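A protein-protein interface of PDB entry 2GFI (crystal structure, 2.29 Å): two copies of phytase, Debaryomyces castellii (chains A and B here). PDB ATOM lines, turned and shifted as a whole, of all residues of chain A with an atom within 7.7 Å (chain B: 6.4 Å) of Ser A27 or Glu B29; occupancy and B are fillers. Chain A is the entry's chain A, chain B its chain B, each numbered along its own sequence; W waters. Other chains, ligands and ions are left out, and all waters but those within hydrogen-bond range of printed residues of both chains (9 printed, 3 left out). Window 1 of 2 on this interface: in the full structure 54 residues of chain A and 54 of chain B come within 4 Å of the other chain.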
ATOM      1  N   LEU A  10       4.228 -12.021 -21.625  1.00  0.00           N
ATOM      2  CA  LEU A  10       5.315 -11.576 -20.750  1.00  0.00           C
ATOM      3  C   LEU A  10       6.649 -12.187 -21.160  1.00  0.00           C
ATOM      4  O   LEU A  10       6.776 -13.389 -21.342  1.00  0.00           O
ATOM      5  CB  LEU A  10       5.020 -11.883 -19.270  1.00  0.00           C
ATOM      6  CG  LEU A  10       3.720 -11.289 -18.735  1.00  0.00           C
ATOM      7  CD1 LEU A  10       3.461 -11.810 -17.335  1.00  0.00           C
ATOM      8  CD2 LEU A  10       3.742  -9.756 -18.769  1.00  0.00           C
ATOM      9  N   VAL A  12       9.209 -12.732 -19.421  1.00  0.00           N
ATOM     10  CA  VAL A  12       9.826 -13.120 -18.157  1.00  0.00           C
ATOM     11  C   VAL A  12       9.137 -14.401 -17.727  1.00  0.00           C
ATOM     12  O   VAL A  12       7.933 -14.592 -18.014  1.00  0.00           O
ATOM     13  CB  VAL A  12       9.629 -12.033 -17.077  1.00  0.00           C
ATOM     14  CG1 VAL A  12       8.116 -11.973 -16.607  1.00  0.00           C
ATOM     15  CG2 VAL A  12      10.624 -12.211 -15.894  1.00  0.00           C
ATOM     16  N   ALA A  16      10.719 -14.431 -11.571  1.00  0.00           N
ATOM     17  CA  ALA A  16      10.371 -13.133 -11.044  1.00  0.00           C
ATOM     18  C   ALA A  16       9.800 -13.231  -9.611  1.00  0.00           C
ATOM     19  O   ALA A  16       9.840 -12.245  -8.857  1.00  0.00           O
ATOM     20  CB  ALA A  16       9.334 -12.446 -11.989  1.00  0.00           C
ATOM     21  N   TYR A  17       9.306 -14.416  -9.249  1.00  0.00           N
ATOM     22  CA  TYR A  17       8.539 -14.613  -8.021  1.00  0.00           C
ATOM     23  C   TYR A  17       9.288 -15.346  -6.950  1.00  0.00           C
ATOM     24  O   TYR A  17       8.755 -15.530  -5.845  1.00  0.00           O
ATOM     25  CB  TYR A  17       7.291 -15.440  -8.315  1.00  0.00           C
ATOM     26  CG  TYR A  17       6.402 -14.781  -9.305  1.00  0.00           C
ATOM     27  CD1 TYR A  17       5.609 -13.680  -8.937  1.00  0.00           C
ATOM     28  CD2 TYR A  17       6.353 -15.222 -10.632  1.00  0.00           C
ATOM     29  CE1 TYR A  17       4.801 -13.062  -9.844  1.00  0.00           C
ATOM     30  CE2 TYR A  17       5.522 -14.584 -11.558  1.00  0.00           C
ATOM     31  CZ  TYR A  17       4.745 -13.522 -11.144  1.00  0.00           C
ATOM     32  OH  TYR A  17       3.900 -12.893 -12.047  1.00  0.00           O
ATOM     33  N   LEU A  20       9.804 -14.049  -3.199  1.00  0.00           N
ATOM     34  CA  LEU A  20       8.790 -13.139  -2.749  1.00  0.00           C
ATOM     35  C   LEU A  20       7.871 -13.905  -1.817  1.00  0.00           C
ATOM     36  O   LEU A  20       7.840 -15.121  -1.853  1.00  0.00           O
ATOM     37  CB  LEU A  20       7.997 -12.597  -3.949  1.00  0.00           C
ATOM     38  CG  LEU A  20       8.782 -11.754  -4.926  1.00  0.00           C
ATOM     39  CD1 LEU A  20       7.878 -11.313  -6.091  1.00  0.00           C
ATOM     40  CD2 LEU A  20       9.464 -10.564  -4.228  1.00  0.00           C
ATOM     41  N   PRO A  23       3.120 -13.009  -4.877  1.00  0.00           N
ATOM     42  CA  PRO A  23       3.375 -12.709  -6.279  1.00  0.00           C
ATOM     43  C   PRO A  23       3.068 -11.246  -6.562  1.00  0.00           C
ATOM     44  O   PRO A  23       3.602 -10.704  -7.516  1.00  0.00           O
ATOM     45  CB  PRO A  23       2.406 -13.651  -7.042  1.00  0.00           C
ATOM     46  CG  PRO A  23       1.423 -14.053  -6.061  1.00  0.00           C
ATOM     47  CD  PRO A  23       2.085 -14.045  -4.726  1.00  0.00           C
ATOM     48  N   GLN A  24       2.247 -10.599  -5.721  1.00  0.00           N
ATOM     49  CA  GLN A  24       1.991  -9.180  -5.904  1.00  0.00           C
ATOM     50  C   GLN A  24       3.182  -8.294  -5.541  1.00  0.00           C
ATOM     51  O   GLN A  24       3.134  -7.091  -5.793  1.00  0.00           O
ATOM     52  CB  GLN A  24       0.733  -8.705  -5.165  1.00  0.00           C
ATOM     53  CG  GLN A  24      -0.503  -9.393  -5.590  1.00  0.00           C
ATOM     54  CD  GLN A  24      -1.706  -9.002  -4.761  1.00  0.00           C
ATOM     55  OE1 GLN A  24      -1.577  -8.418  -3.714  1.00  0.00           O
ATOM     56  NE2 GLN A  24      -2.871  -9.335  -5.230  1.00  0.00           N
ATOM     57  N   GLN A  25       4.250  -8.869  -4.983  1.00  0.00           N
ATOM     58  CA  GLN A  25       5.470  -8.099  -4.763  1.00  0.00           C
ATOM     59  C   GLN A  25       6.289  -8.029  -6.035  1.00  0.00           C
ATOM     60  O   GLN A  25       7.289  -7.342  -6.046  1.00  0.00           O
ATOM     61  CB  GLN A  25       6.323  -8.700  -3.623  1.00  0.00           C
ATOM     62  CG  GLN A  25       5.591  -8.635  -2.256  1.00  0.00           C
ATOM     63  CD  GLN A  25       6.326  -9.379  -1.199  1.00  0.00           C
ATOM     64  OE1 GLN A  25       6.230 -10.606  -1.119  1.00  0.00           O
ATOM     65  NE2 GLN A  25       7.061  -8.659  -0.369  1.00  0.00           N
ATOM     66  N   ALA A  26       5.876  -8.749  -7.083  1.00  0.00           N
ATOM     67  CA  ALA A  26       6.631  -8.826  -8.333  1.00  0.00           C
ATOM     68  C   ALA A  26       6.253  -7.720  -9.265  1.00  0.00           C
ATOM     69  O   ALA A  26       5.090  -7.289  -9.293  1.00  0.00           O
ATOM     70  CB  ALA A  26       6.395 -10.157  -9.039  1.00  0.00           C
ATOM     71  N   SER A  27       7.223  -7.270 -10.051  1.00  0.00           N
ATOM     72  CA  SER A  27       6.929  -6.344 -11.136  1.00  0.00           C
ATOM     73  C   SER A  27       7.192  -7.028 -12.469  1.00  0.00           C
ATOM     74  O   SER A  27       8.335  -7.073 -12.953  1.00  0.00           O
ATOM     75  CB  SER A  27       7.724  -5.045 -10.994  1.00  0.00           C
ATOM     76  OG  SER A  27       7.408  -4.465  -9.741  1.00  0.00           O
ATOM     77  N   VAL A  28       6.139  -7.571 -13.057  1.00  0.00           N
ATOM     78  CA  VAL A  28       6.292  -8.339 -14.289  1.00  0.00           C
ATOM     79  C   VAL A  28       5.719  -7.595 -15.481  1.00  0.00           C
ATOM     80  O   VAL A  28       6.069  -7.905 -16.600  1.00  0.00           O
ATOM     81  CB  VAL A  28       5.686  -9.751 -14.174  1.00  0.00           C
ATOM     82  CG1 VAL A  28       6.505 -10.590 -13.187  1.00  0.00           C
ATOM     83  CG2 VAL A  28       4.198  -9.703 -13.774  1.00  0.00           C
ATOM     84  N   GLU A  29       4.892  -6.576 -15.230  1.00  0.00           N
ATOM     85  CA  GLU A  29       4.246  -5.798 -16.319  1.00  0.00           C
ATOM     86  C   GLU A  29       5.232  -5.083 -17.225  1.00  0.00           C
ATOM     87  O   GLU A  29       4.929  -4.855 -18.388  1.00  0.00           O
ATOM     88  CB  GLU A  29       3.216  -4.808 -15.759  1.00  0.00           C
ATOM     89  CG  GLU A  29       1.991  -5.539 -15.254  1.00  0.00           C
ATOM     90  CD  GLU A  29       1.035  -4.658 -14.472  1.00  0.00           C
ATOM     91  OE1 GLU A  29       1.241  -3.413 -14.435  1.00  0.00           O
ATOM     92  OE2 GLU A  29       0.066  -5.218 -13.907  1.00  0.00           O
ATOM     93  N   GLN A  30       6.402  -4.729 -16.696  1.00  0.00           N
ATOM     94  CA  GLN A  30       7.470  -4.133 -17.512  1.00  0.00           C
ATOM     95  C   GLN A  30       7.832  -5.068 -18.686  1.00  0.00           C
ATOM     96  O   GLN A  30       8.390  -4.630 -19.681  1.00  0.00           O
ATOM     97  CB  GLN A  30       8.716  -3.887 -16.652  1.00  0.00           C
ATOM     98  CG  GLN A  30       9.111  -5.140 -15.901  1.00  0.00           C
ATOM     99  CD  GLN A  30      10.369  -5.042 -15.083  1.00  0.00           C
ATOM    100  OE1 GLN A  30      10.354  -5.377 -13.877  1.00  0.00           O
ATOM    101  NE2 GLN A  30      11.449  -4.618 -15.694  1.00  0.00           N
ATOM    102  N   TYR A  31       7.515  -6.352 -18.558  1.00  0.00           N
ATOM    103  CA  TYR A  31       8.008  -7.353 -19.503  1.00  0.00           C
ATOM    104  C   TYR A  31       6.999  -7.675 -20.600  1.00  0.00           C
ATOM    105  O   TYR A  31       7.222  -8.550 -21.407  1.00  0.00           O
ATOM    106  CB  TYR A  31       8.360  -8.644 -18.770  1.00  0.00           C
ATOM    107  CG  TYR A  31       9.530  -8.532 -17.841  1.00  0.00           C
ATOM    108  CD1 TYR A  31      10.812  -8.302 -18.322  1.00  0.00           C
ATOM    109  CD2 TYR A  31       9.360  -8.692 -16.452  1.00  0.00           C
ATOM    110  CE1 TYR A  31      11.899  -8.234 -17.452  1.00  0.00           C
ATOM    111  CE2 TYR A  31      10.422  -8.650 -15.586  1.00  0.00           C
ATOM    112  CZ  TYR A  31      11.683  -8.427 -16.096  1.00  0.00           C
ATOM    113  OH  TYR A  31      12.727  -8.367 -15.229  1.00  0.00           O
ATOM    114  N   ARG A  35       4.371  -3.749 -24.986  1.00  0.00           N
ATOM    115  CA  ARG A  35       4.919  -2.442 -24.694  1.00  0.00           C
ATOM    116  C   ARG A  35       6.134  -2.143 -25.569  1.00  0.00           C
ATOM    117  O   ARG A  35       6.551  -0.995 -25.641  1.00  0.00           O
ATOM    118  CB  ARG A  35       5.179  -2.216 -23.171  1.00  0.00           C
ATOM    119  CG  ARG A  35       3.852  -2.107 -22.374  1.00  0.00           C
ATOM    120  CD  ARG A  35       3.689  -0.956 -21.324  1.00  0.00           C
ATOM    121  NE  ARG A  35       2.462  -1.145 -20.504  1.00  0.00           N
ATOM    122  CZ  ARG A  35       2.319  -2.210 -19.665  1.00  0.00           C
ATOM    123  NH1 ARG A  35       3.321  -3.114 -19.576  1.00  0.00           N
ATOM    124  NH2 ARG A  35       1.217  -2.392 -18.918  1.00  0.00           N
ATOM    125  N   LYS A  47       0.697   2.096 -18.011  1.00  0.00           N
ATOM    126  CA  LYS A  47       1.267   1.664 -16.710  1.00  0.00           C
ATOM    127  C   LYS A  47       0.607   2.429 -15.542  1.00  0.00           C
ATOM    128  O   LYS A  47       0.306   1.838 -14.519  1.00  0.00           O
ATOM    129  CB  LYS A  47       2.795   1.758 -16.682  1.00  0.00           C
ATOM    130  CG  LYS A  47       3.505   1.000 -17.860  1.00  0.00           C
ATOM    131  CD  LYS A  47       5.085   1.127 -17.813  1.00  0.00           C
ATOM    132  CE  LYS A  47       5.757  -0.185 -18.367  1.00  0.00           C
ATOM    133  NZ  LYS A  47       7.254  -0.295 -18.154  1.00  0.00           N
ATOM    134  N   GLY A  48       0.349   3.724 -15.735  1.00  0.00           N
ATOM    135  CA  GLY A  48      -0.440   4.541 -14.796  1.00  0.00           C
ATOM    136  C   GLY A  48       0.220   4.846 -13.467  1.00  0.00           C
ATOM    137  O   GLY A  48       1.386   4.562 -13.302  1.00  0.00           O
ATOM    138  N   PHE A  49      -0.515   5.423 -12.511  1.00  0.00           N
ATOM    139  CA  PHE A  49       0.143   5.918 -11.294  1.00  0.00           C
ATOM    140  C   PHE A  49      -0.555   5.478 -10.035  1.00  0.00           C
ATOM    141  O   PHE A  49      -0.197   5.934  -8.953  1.00  0.00           O
ATOM    142  CB  PHE A  49       0.253   7.444 -11.271  1.00  0.00           C
ATOM    143  CG  PHE A  49       0.883   8.035 -12.496  1.00  0.00           C
ATOM    144  CD1 PHE A  49       2.257   7.919 -12.725  1.00  0.00           C
ATOM    145  CD2 PHE A  49       0.099   8.758 -13.414  1.00  0.00           C
ATOM    146  CE1 PHE A  49       2.826   8.491 -13.864  1.00  0.00           C
ATOM    147  CE2 PHE A  49       0.661   9.345 -14.539  1.00  0.00           C
ATOM    148  CZ  PHE A  49       2.025   9.214 -14.768  1.00  0.00           C
ATOM    149  N   GLY A  50      -1.569   4.611 -10.167  1.00  0.00           N
ATOM    150  CA  GLY A  50      -2.249   4.081  -9.002  1.00  0.00           C
ATOM    151  C   GLY A  50      -3.481   4.868  -8.644  1.00  0.00           C
ATOM    152  O   GLY A  50      -4.107   4.582  -7.646  1.00  0.00           O
ATOM    153  N   LEU B  10      -3.306  -4.905  -3.582  1.00  0.00           N
ATOM    154  CA  LEU B  10      -3.728  -4.089  -4.706  1.00  0.00           C
ATOM    155  C   LEU B  10      -4.942  -3.232  -4.406  1.00  0.00           C
ATOM    156  O   LEU B  10      -5.982  -3.731  -3.948  1.00  0.00           O
ATOM    157  CB  LEU B  10      -3.968  -4.950  -5.937  1.00  0.00           C
ATOM    158  CG  LEU B  10      -2.749  -5.680  -6.522  1.00  0.00           C
ATOM    159  CD1 LEU B  10      -3.290  -6.533  -7.690  1.00  0.00           C
ATOM    160  CD2 LEU B  10      -1.629  -4.770  -7.010  1.00  0.00           C
ATOM    161  N   VAL B  12      -6.994  -1.936  -6.327  1.00  0.00           N
ATOM    162  CA  VAL B  12      -7.864  -1.998  -7.500  1.00  0.00           C
ATOM    163  C   VAL B  12      -8.641  -3.327  -7.423  1.00  0.00           C
ATOM    164  O   VAL B  12      -8.223  -4.268  -6.776  1.00  0.00           O
ATOM    165  CB  VAL B  12      -7.031  -1.866  -8.824  1.00  0.00           C
ATOM    166  CG1 VAL B  12      -6.046  -3.094  -8.998  1.00  0.00           C
ATOM    167  CG2 VAL B  12      -7.928  -1.640 -10.047  1.00  0.00           C
ATOM    168  N   ALA B  26      -3.791  -5.823 -18.629  1.00  0.00           N
ATOM    169  CA  ALA B  26      -4.065  -4.925 -17.496  1.00  0.00           C
ATOM    170  C   ALA B  26      -2.810  -4.442 -16.891  1.00  0.00           C
ATOM    171  O   ALA B  26      -1.831  -5.203 -16.794  1.00  0.00           O
ATOM    172  CB  ALA B  26      -4.903  -5.636 -16.393  1.00  0.00           C
ATOM    173  N   SER B  27      -2.852  -3.191 -16.441  1.00  0.00           N
ATOM    174  CA  SER B  27      -1.783  -2.642 -15.603  1.00  0.00           C
ATOM    175  C   SER B  27      -2.297  -2.463 -14.182  1.00  0.00           C
ATOM    176  O   SER B  27      -3.019  -1.503 -13.888  1.00  0.00           O
ATOM    177  CB  SER B  27      -1.316  -1.296 -16.145  1.00  0.00           C
ATOM    178  OG  SER B  27      -0.803  -1.462 -17.427  1.00  0.00           O
ATOM    179  N   VAL B  28      -1.989  -3.398 -13.317  1.00  0.00           N
ATOM    180  CA  VAL B  28      -2.504  -3.302 -11.958  1.00  0.00           C
ATOM    181  C   VAL B  28      -1.445  -3.061 -10.913  1.00  0.00           C
ATOM    182  O   VAL B  28      -1.770  -2.753  -9.754  1.00  0.00           O
ATOM    183  CB  VAL B  28      -3.355  -4.512 -11.563  1.00  0.00           C
ATOM    184  CG1 VAL B  28      -4.527  -4.630 -12.520  1.00  0.00           C
ATOM    185  CG2 VAL B  28      -2.522  -5.771 -11.534  1.00  0.00           C
ATOM    186  N   GLU B  29      -0.186  -3.156 -11.326  1.00  0.00           N
ATOM    187  CA  GLU B  29       0.933  -3.001 -10.430  1.00  0.00           C
ATOM    188  C   GLU B  29       1.028  -1.633  -9.825  1.00  0.00           C
ATOM    189  O   GLU B  29       1.486  -1.490  -8.684  1.00  0.00           O
ATOM    190  CB  GLU B  29       2.241  -3.379 -11.131  1.00  0.00           C
ATOM    191  CG  GLU B  29       2.366  -4.902 -11.219  1.00  0.00           C
ATOM    192  CD  GLU B  29       3.517  -5.368 -12.097  1.00  0.00           C
ATOM    193  OE1 GLU B  29       4.315  -4.488 -12.555  1.00  0.00           O
ATOM    194  OE2 GLU B  29       3.606  -6.607 -12.308  1.00  0.00           O
ATOM    195  N   GLN B  30       0.606  -0.640 -10.610  1.00  0.00           N
ATOM    196  CA  GLN B  30       0.555   0.751 -10.204  1.00  0.00           C
ATOM    197  C   GLN B  30      -0.235   0.945  -8.884  1.00  0.00           C
ATOM    198  O   GLN B  30      -0.037   1.930  -8.181  1.00  0.00           O
ATOM    199  CB  GLN B  30      -0.108   1.584 -11.335  1.00  0.00           C
ATOM    200  CG  GLN B  30      -1.530   1.039 -11.778  1.00  0.00           C
ATOM    201  CD  GLN B  30      -2.318   1.987 -12.691  1.00  0.00           C
ATOM    202  OE1 GLN B  30      -2.411   3.190 -12.413  1.00  0.00           O
ATOM    203  NE2 GLN B  30      -2.906   1.446 -13.778  1.00  0.00           N
ATOM    204  N   TYR B  31      -1.146   0.020  -8.592  1.00  0.00           N
ATOM    205  CA  TYR B  31      -2.103   0.123  -7.477  1.00  0.00           C
ATOM    206  C   TYR B  31      -1.602  -0.594  -6.257  1.00  0.00           C
ATOM    207  O   TYR B  31      -2.308  -0.684  -5.242  1.00  0.00           O
ATOM    208  CB  TYR B  31      -3.422  -0.544  -7.849  1.00  0.00           C
ATOM    209  CG  TYR B  31      -4.157   0.166  -8.939  1.00  0.00           C
ATOM    210  CD1 TYR B  31      -4.712   1.402  -8.716  1.00  0.00           C
ATOM    211  CD2 TYR B  31      -4.277  -0.405 -10.215  1.00  0.00           C
ATOM    212  CE1 TYR B  31      -5.378   2.056  -9.694  1.00  0.00           C
ATOM    213  CE2 TYR B  31      -4.951   0.248 -11.224  1.00  0.00           C
ATOM    214  CZ  TYR B  31      -5.514   1.477 -10.949  1.00  0.00           C
ATOM    215  OH  TYR B  31      -6.171   2.171 -11.926  1.00  0.00           O
ATOM    216  N   ASN B  32      -0.405  -1.148  -6.346  1.00  0.00           N
ATOM    217  CA  ASN B  32       0.142  -1.797  -5.182  1.00  0.00           C
ATOM    218  C   ASN B  32       0.357  -0.858  -4.007  1.00  0.00           C
ATOM    219  O   ASN B  32       1.143   0.127  -4.089  1.00  0.00           O
ATOM    220  CB  ASN B  32       1.406  -2.573  -5.490  1.00  0.00           C
ATOM    221  CG  ASN B  32       1.706  -3.564  -4.415  1.00  0.00           C
ATOM    222  OD1 ASN B  32       1.960  -3.201  -3.273  1.00  0.00           O
ATOM    223  ND2 ASN B  32       1.617  -4.817  -4.747  1.00  0.00           N
ATOM    224  N   ILE B  33      -0.353  -1.138  -2.920  1.00  0.00           N
ATOM    225  CA  ILE B  33      -0.268  -0.273  -1.742  1.00  0.00           C
ATOM    226  C   ILE B  33       1.155   0.002  -1.277  1.00  0.00           C
ATOM    227  O   ILE B  33       1.478   1.094  -0.823  1.00  0.00           O
ATOM    228  CB  ILE B  33      -1.111  -0.838  -0.542  1.00  0.00           C
ATOM    229  CG1 ILE B  33      -1.308   0.287   0.506  1.00  0.00           C
ATOM    230  CG2 ILE B  33      -0.480  -2.169   0.003  1.00  0.00           C
ATOM    231  CD1 ILE B  33      -2.279  -0.056   1.631  1.00  0.00           C
ATOM    232  N   ARG B  35       3.728   0.639  -2.812  1.00  0.00           N
ATOM    233  CA  ARG B  35       4.412   1.710  -3.487  1.00  0.00           C
ATOM    234  C   ARG B  35       4.073   3.077  -2.865  1.00  0.00           C
ATOM    235  O   ARG B  35       4.763   4.084  -3.146  1.00  0.00           O
ATOM    236  CB  ARG B  35       4.057   1.721  -4.958  1.00  0.00           C
ATOM    237  CG  ARG B  35       5.007   0.949  -5.851  1.00  0.00           C
ATOM    238  CD  ARG B  35       4.444   0.797  -7.261  1.00  0.00           C
ATOM    239  NE  ARG B  35       4.471  -0.602  -7.736  1.00  0.00           N
ATOM    240  CZ  ARG B  35       5.590  -1.273  -7.860  1.00  0.00           C
ATOM    241  NH1 ARG B  35       6.743  -0.671  -7.535  1.00  0.00           N
ATOM    242  NH2 ARG B  35       5.556  -2.529  -8.281  1.00  0.00           N
ATOM    243  N   ILE B  44       8.956  -4.712  -2.452  1.00  0.00           N
ATOM    244  CA  ILE B  44       8.319  -4.789  -3.741  1.00  0.00           C
ATOM    245  C   ILE B  44       9.398  -4.507  -4.772  1.00  0.00           C
ATOM    246  O   ILE B  44      10.289  -3.658  -4.557  1.00  0.00           O
ATOM    247  CB  ILE B  44       7.142  -3.777  -3.856  1.00  0.00           C
ATOM    248  CG1 ILE B  44       6.350  -4.014  -5.130  1.00  0.00           C
ATOM    249  CG2 ILE B  44       7.628  -2.280  -3.781  1.00  0.00           C
ATOM    250  CD1 ILE B  44       4.992  -3.301  -5.077  1.00  0.00           C
ATOM    251  N   GLN B  45       9.309  -5.230  -5.889  1.00  0.00           N
ATOM    252  CA  GLN B  45      10.252  -5.049  -6.985  1.00  0.00           C
ATOM    253  C   GLN B  45      10.062  -3.687  -7.652  1.00  0.00           C
ATOM    254  O   GLN B  45       8.962  -3.143  -7.722  1.00  0.00           O
ATOM    255  CB  GLN B  45      10.137  -6.184  -7.991  1.00  0.00           C
ATOM    256  CG  GLN B  45      10.451  -7.561  -7.412  1.00  0.00           C
ATOM    257  CD  GLN B  45      10.280  -8.687  -8.418  1.00  0.00           C
ATOM    258  OE1 GLN B  45       9.606  -8.516  -9.430  1.00  0.00           O
ATOM    259  NE2 GLN B  45      10.903  -9.829  -8.157  1.00  0.00           N
ATOM    260  N   ASN B  46      11.160  -3.129  -8.131  1.00  0.00           N
ATOM    261  CA  ASN B  46      11.121  -1.921  -8.894  1.00  0.00           C
ATOM    262  C   ASN B  46      10.275  -2.147 -10.133  1.00  0.00           C
ATOM    263  O   ASN B  46      10.323  -3.211 -10.731  1.00  0.00           O
ATOM    264  CB  ASN B  46      12.562  -1.540  -9.256  1.00  0.00           C
ATOM    265  CG  ASN B  46      12.659  -0.184  -9.874  1.00  0.00           C
ATOM    266  OD1 ASN B  46      12.290  -0.006 -11.021  1.00  0.00           O
ATOM    267  ND2 ASN B  46      13.187   0.785  -9.128  1.00  0.00           N
ATOM    268  N   LYS B  47       9.500  -1.155 -10.526  1.00  0.00           N
ATOM    269  CA  LYS B  47       8.703  -1.245 -11.761  1.00  0.00           C
ATOM    270  C   LYS B  47       9.508  -1.710 -12.962  1.00  0.00           C
ATOM    271  O   LYS B  47       9.032  -2.513 -13.730  1.00  0.00           O
ATOM    272  CB  LYS B  47       8.014   0.085 -12.074  1.00  0.00           C
ATOM    273  CG  LYS B  47       6.785   0.353 -11.246  1.00  0.00           C
ATOM    274  CD  LYS B  47       6.239   1.753 -11.596  1.00  0.00           C
ATOM    275  CE  LYS B  47       5.495   2.391 -10.373  1.00  0.00           C
ATOM    276  NZ  LYS B  47       4.011   2.171 -10.342  1.00  0.00           N
ATOM    277  N   GLY B  48      10.708  -1.173 -13.144  1.00  0.00           N
ATOM    278  CA  GLY B  48      11.634  -1.672 -14.160  1.00  0.00           C
ATOM    279  C   GLY B  48      11.233  -1.267 -15.557  1.00  0.00           C
ATOM    280  O   GLY B  48      10.228  -0.586 -15.741  1.00  0.00           O
ATOM    281  N   ASN B 393      16.185  -3.559  -6.972  1.00  0.00           N
ATOM    282  CA  ASN B 393      14.948  -4.264  -6.628  1.00  0.00           C
ATOM    283  C   ASN B 393      14.427  -5.080  -7.802  1.00  0.00           C
ATOM    284  O   ASN B 393      13.262  -4.967  -8.211  1.00  0.00           O
ATOM    285  CB  ASN B 393      13.923  -3.332  -5.977  1.00  0.00           C
ATOM    286  CG  ASN B 393      14.542  -2.531  -4.842  1.00  0.00           C
ATOM    287  OD1 ASN B 393      14.521  -1.304  -4.842  1.00  0.00           O
ATOM    288  ND2 ASN B 393      15.119  -3.218  -3.891  1.00  0.00           N
ATOM    289  N   ASP B 394      15.363  -5.868  -8.347  1.00  0.00           N
ATOM    290  CA  ASP B 394      15.108  -6.870  -9.364  1.00  0.00           C
ATOM    291  C   ASP B 394      14.784  -6.274 -10.703  1.00  0.00           C
ATOM    292  O   ASP B 394      14.205  -6.962 -11.523  1.00  0.00           O
ATOM    293  CB  ASP B 394      13.967  -7.816  -8.929  1.00  0.00           C
ATOM    294  CG  ASP B 394      14.308  -8.595  -7.669  1.00  0.00           C
ATOM    295  OD1 ASP B 394      15.368  -9.293  -7.649  1.00  0.00           O
ATOM    296  OD2 ASP B 394      13.571  -8.582  -6.659  1.00  0.00           O
HETATM  297  O   HOH W   1      -2.993   6.533 -12.764  1.00  0.00           O
HETATM  298  O   HOH W   2       0.932  -7.498 -12.692  1.00  0.00           O
HETATM  299  O   HOH W   3       2.096   3.299  -8.808  1.00  0.00           O
HETATM  300  O   HOH W   4       1.685  -5.458  -7.646  1.00  0.00           O
HETATM  301  O   HOH W   5       4.281  -4.798  -8.315  1.00  0.00           O
HETATM  302  O   HOH W   6      10.045  -9.055 -12.012  1.00  0.00           O
HETATM  303  O   HOH W   7       0.394  -0.679 -13.547  1.00  0.00           O
HETATM  304  O   HOH W   8       0.559  -4.913 -18.318  1.00  0.00           O
HETATM  305  O   HOH W   9      12.341  -8.353 -12.710  1.00  0.00           O
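Positions printed for both chains: 10, 12, 26, 27, 28, 29, 30, 31, 35, 47 and 48.
Of the 29 pairs that touch across the chains among the printed residues, 15 have their exchanged pair printed and touching as well.
Val A12 touches none of the printed residues of chain B.
Of chain B, only Glu B29, Arg B35, Gln B45, Asn B46 and Lys B47 come within 4 Å of Ser A27.
Printed residues of chain B within 4 Å of Arg A35: Ser B27 (2.7 Å).
Glu B29 touches four residues of chain A.
Printed residues of chain A within 4 Å of Ile B44: Gln A25 (3.6 Å).
The nearest residue of chain B that does not touch Ser A27 is Ile B44 (4.8 Å).
The nearest printed residue of chain B that does not touch Leu A20 is Asp B394 (5.2 Å).
Water W9 lies within hydrogen-bond range of OH of Tyr A31 and O of Asp B394.
Water W2 lies within hydrogen-bond range of the side-chain carboxylate (OE2) of Glu A29 (2.7 Å) and the side-chain carboxylate (OE2) of Glu B29 (2.8 Å).
The guanidinium group (NH1) of Arg B35 is in hydrogen-bond range of the backbone carbonyl oxygen (O) of Gln B45, at 3.3 Å.
O of Ser A27 sits close to OE1 of Gln A30, 2.8 Å away.
O of Ser B27 is in hydrogen-bond range of NE2 of Gln B30, at 3.0 Å.
O of Gln A25 sits at hydrogen-bond distance from N of Gln B45, 2.9 Å away.
O of Gln A24 lies within hydrogen-bond range of ND2 of Asn B32, 2.9 Å away.
The side-chain carboxylate (OE2) of Glu B29 is in hydrogen-bond range of the backbone NH (N) of Glu A29, 3.2 Å away.
OG of Ser A27 lies close to O of Asn B46 (3.3 Å).
N of Gly A50 lies within hydrogen-bond range of OE1 of Gln B30 (2.8 Å).
O of Lys A47 sits close to NE2 of Gln B30, 3.3 Å away.
The backbone NH of Ser A27 is in hydrogen-bond range of the side-chain amide oxygen of Gln B45 (2.8 Å).
OE1 of Gln A30 lies close to O of Lys B47 (3.2 Å).
The backbone NH (N) of Val B28 is in hydrogen-bond range of the side-chain carboxylate (OE2) of Glu A29, at 2.8 Å.
The guanidinium group of Arg A35 sits at hydrogen-bond distance from the side-chain hydroxyl of Ser B27.
The side-chain amide nitrogen (NE2) of Gln B45 sits at hydrogen-bond distance from the backbone carbonyl oxygen (O) of Ala A16 (2.7 Å).
O of Ala B26 lies close to OE2 of Glu A29 (3.5 Å).
The side-chain amide oxygen of Gln B30 is in hydrogen-bond range of the backbone NH of Phe A49 (2.9 Å).
The backbone NH of Val A28 is in hydrogen-bond range of the side-chain carboxylate of Glu B29 (2.8 Å).
The backbone carbonyl oxygen (O) of Ala A26 lies close to the side-chain carboxylate (OE2) of Glu B29.
OG of Ser A27 sits at hydrogen-bond distance from NH2 of Arg B35 (3.1 Å).
Hydrophobic or aromatic side chains of chain B within 4 Å of the printed part of chain A: Leu B10, Val B28, Tyr B31 and Ile B44.
Along chain B the printed residues that touch a printed residue of chain A span positions 10 to 48.
Of the 19 printed residues of chain A, 14 touch a printed residue of chain B.
Hydrophobic or aromatic side chains of chain A within 4 Å of the printed part of chain B: Leu A20, Ala A26 and Val A28.
Along chain A the printed residues that touch a printed residue of chain B span positions 16 to 50.
Among the printed residues, 29 pairs touch across the chains.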
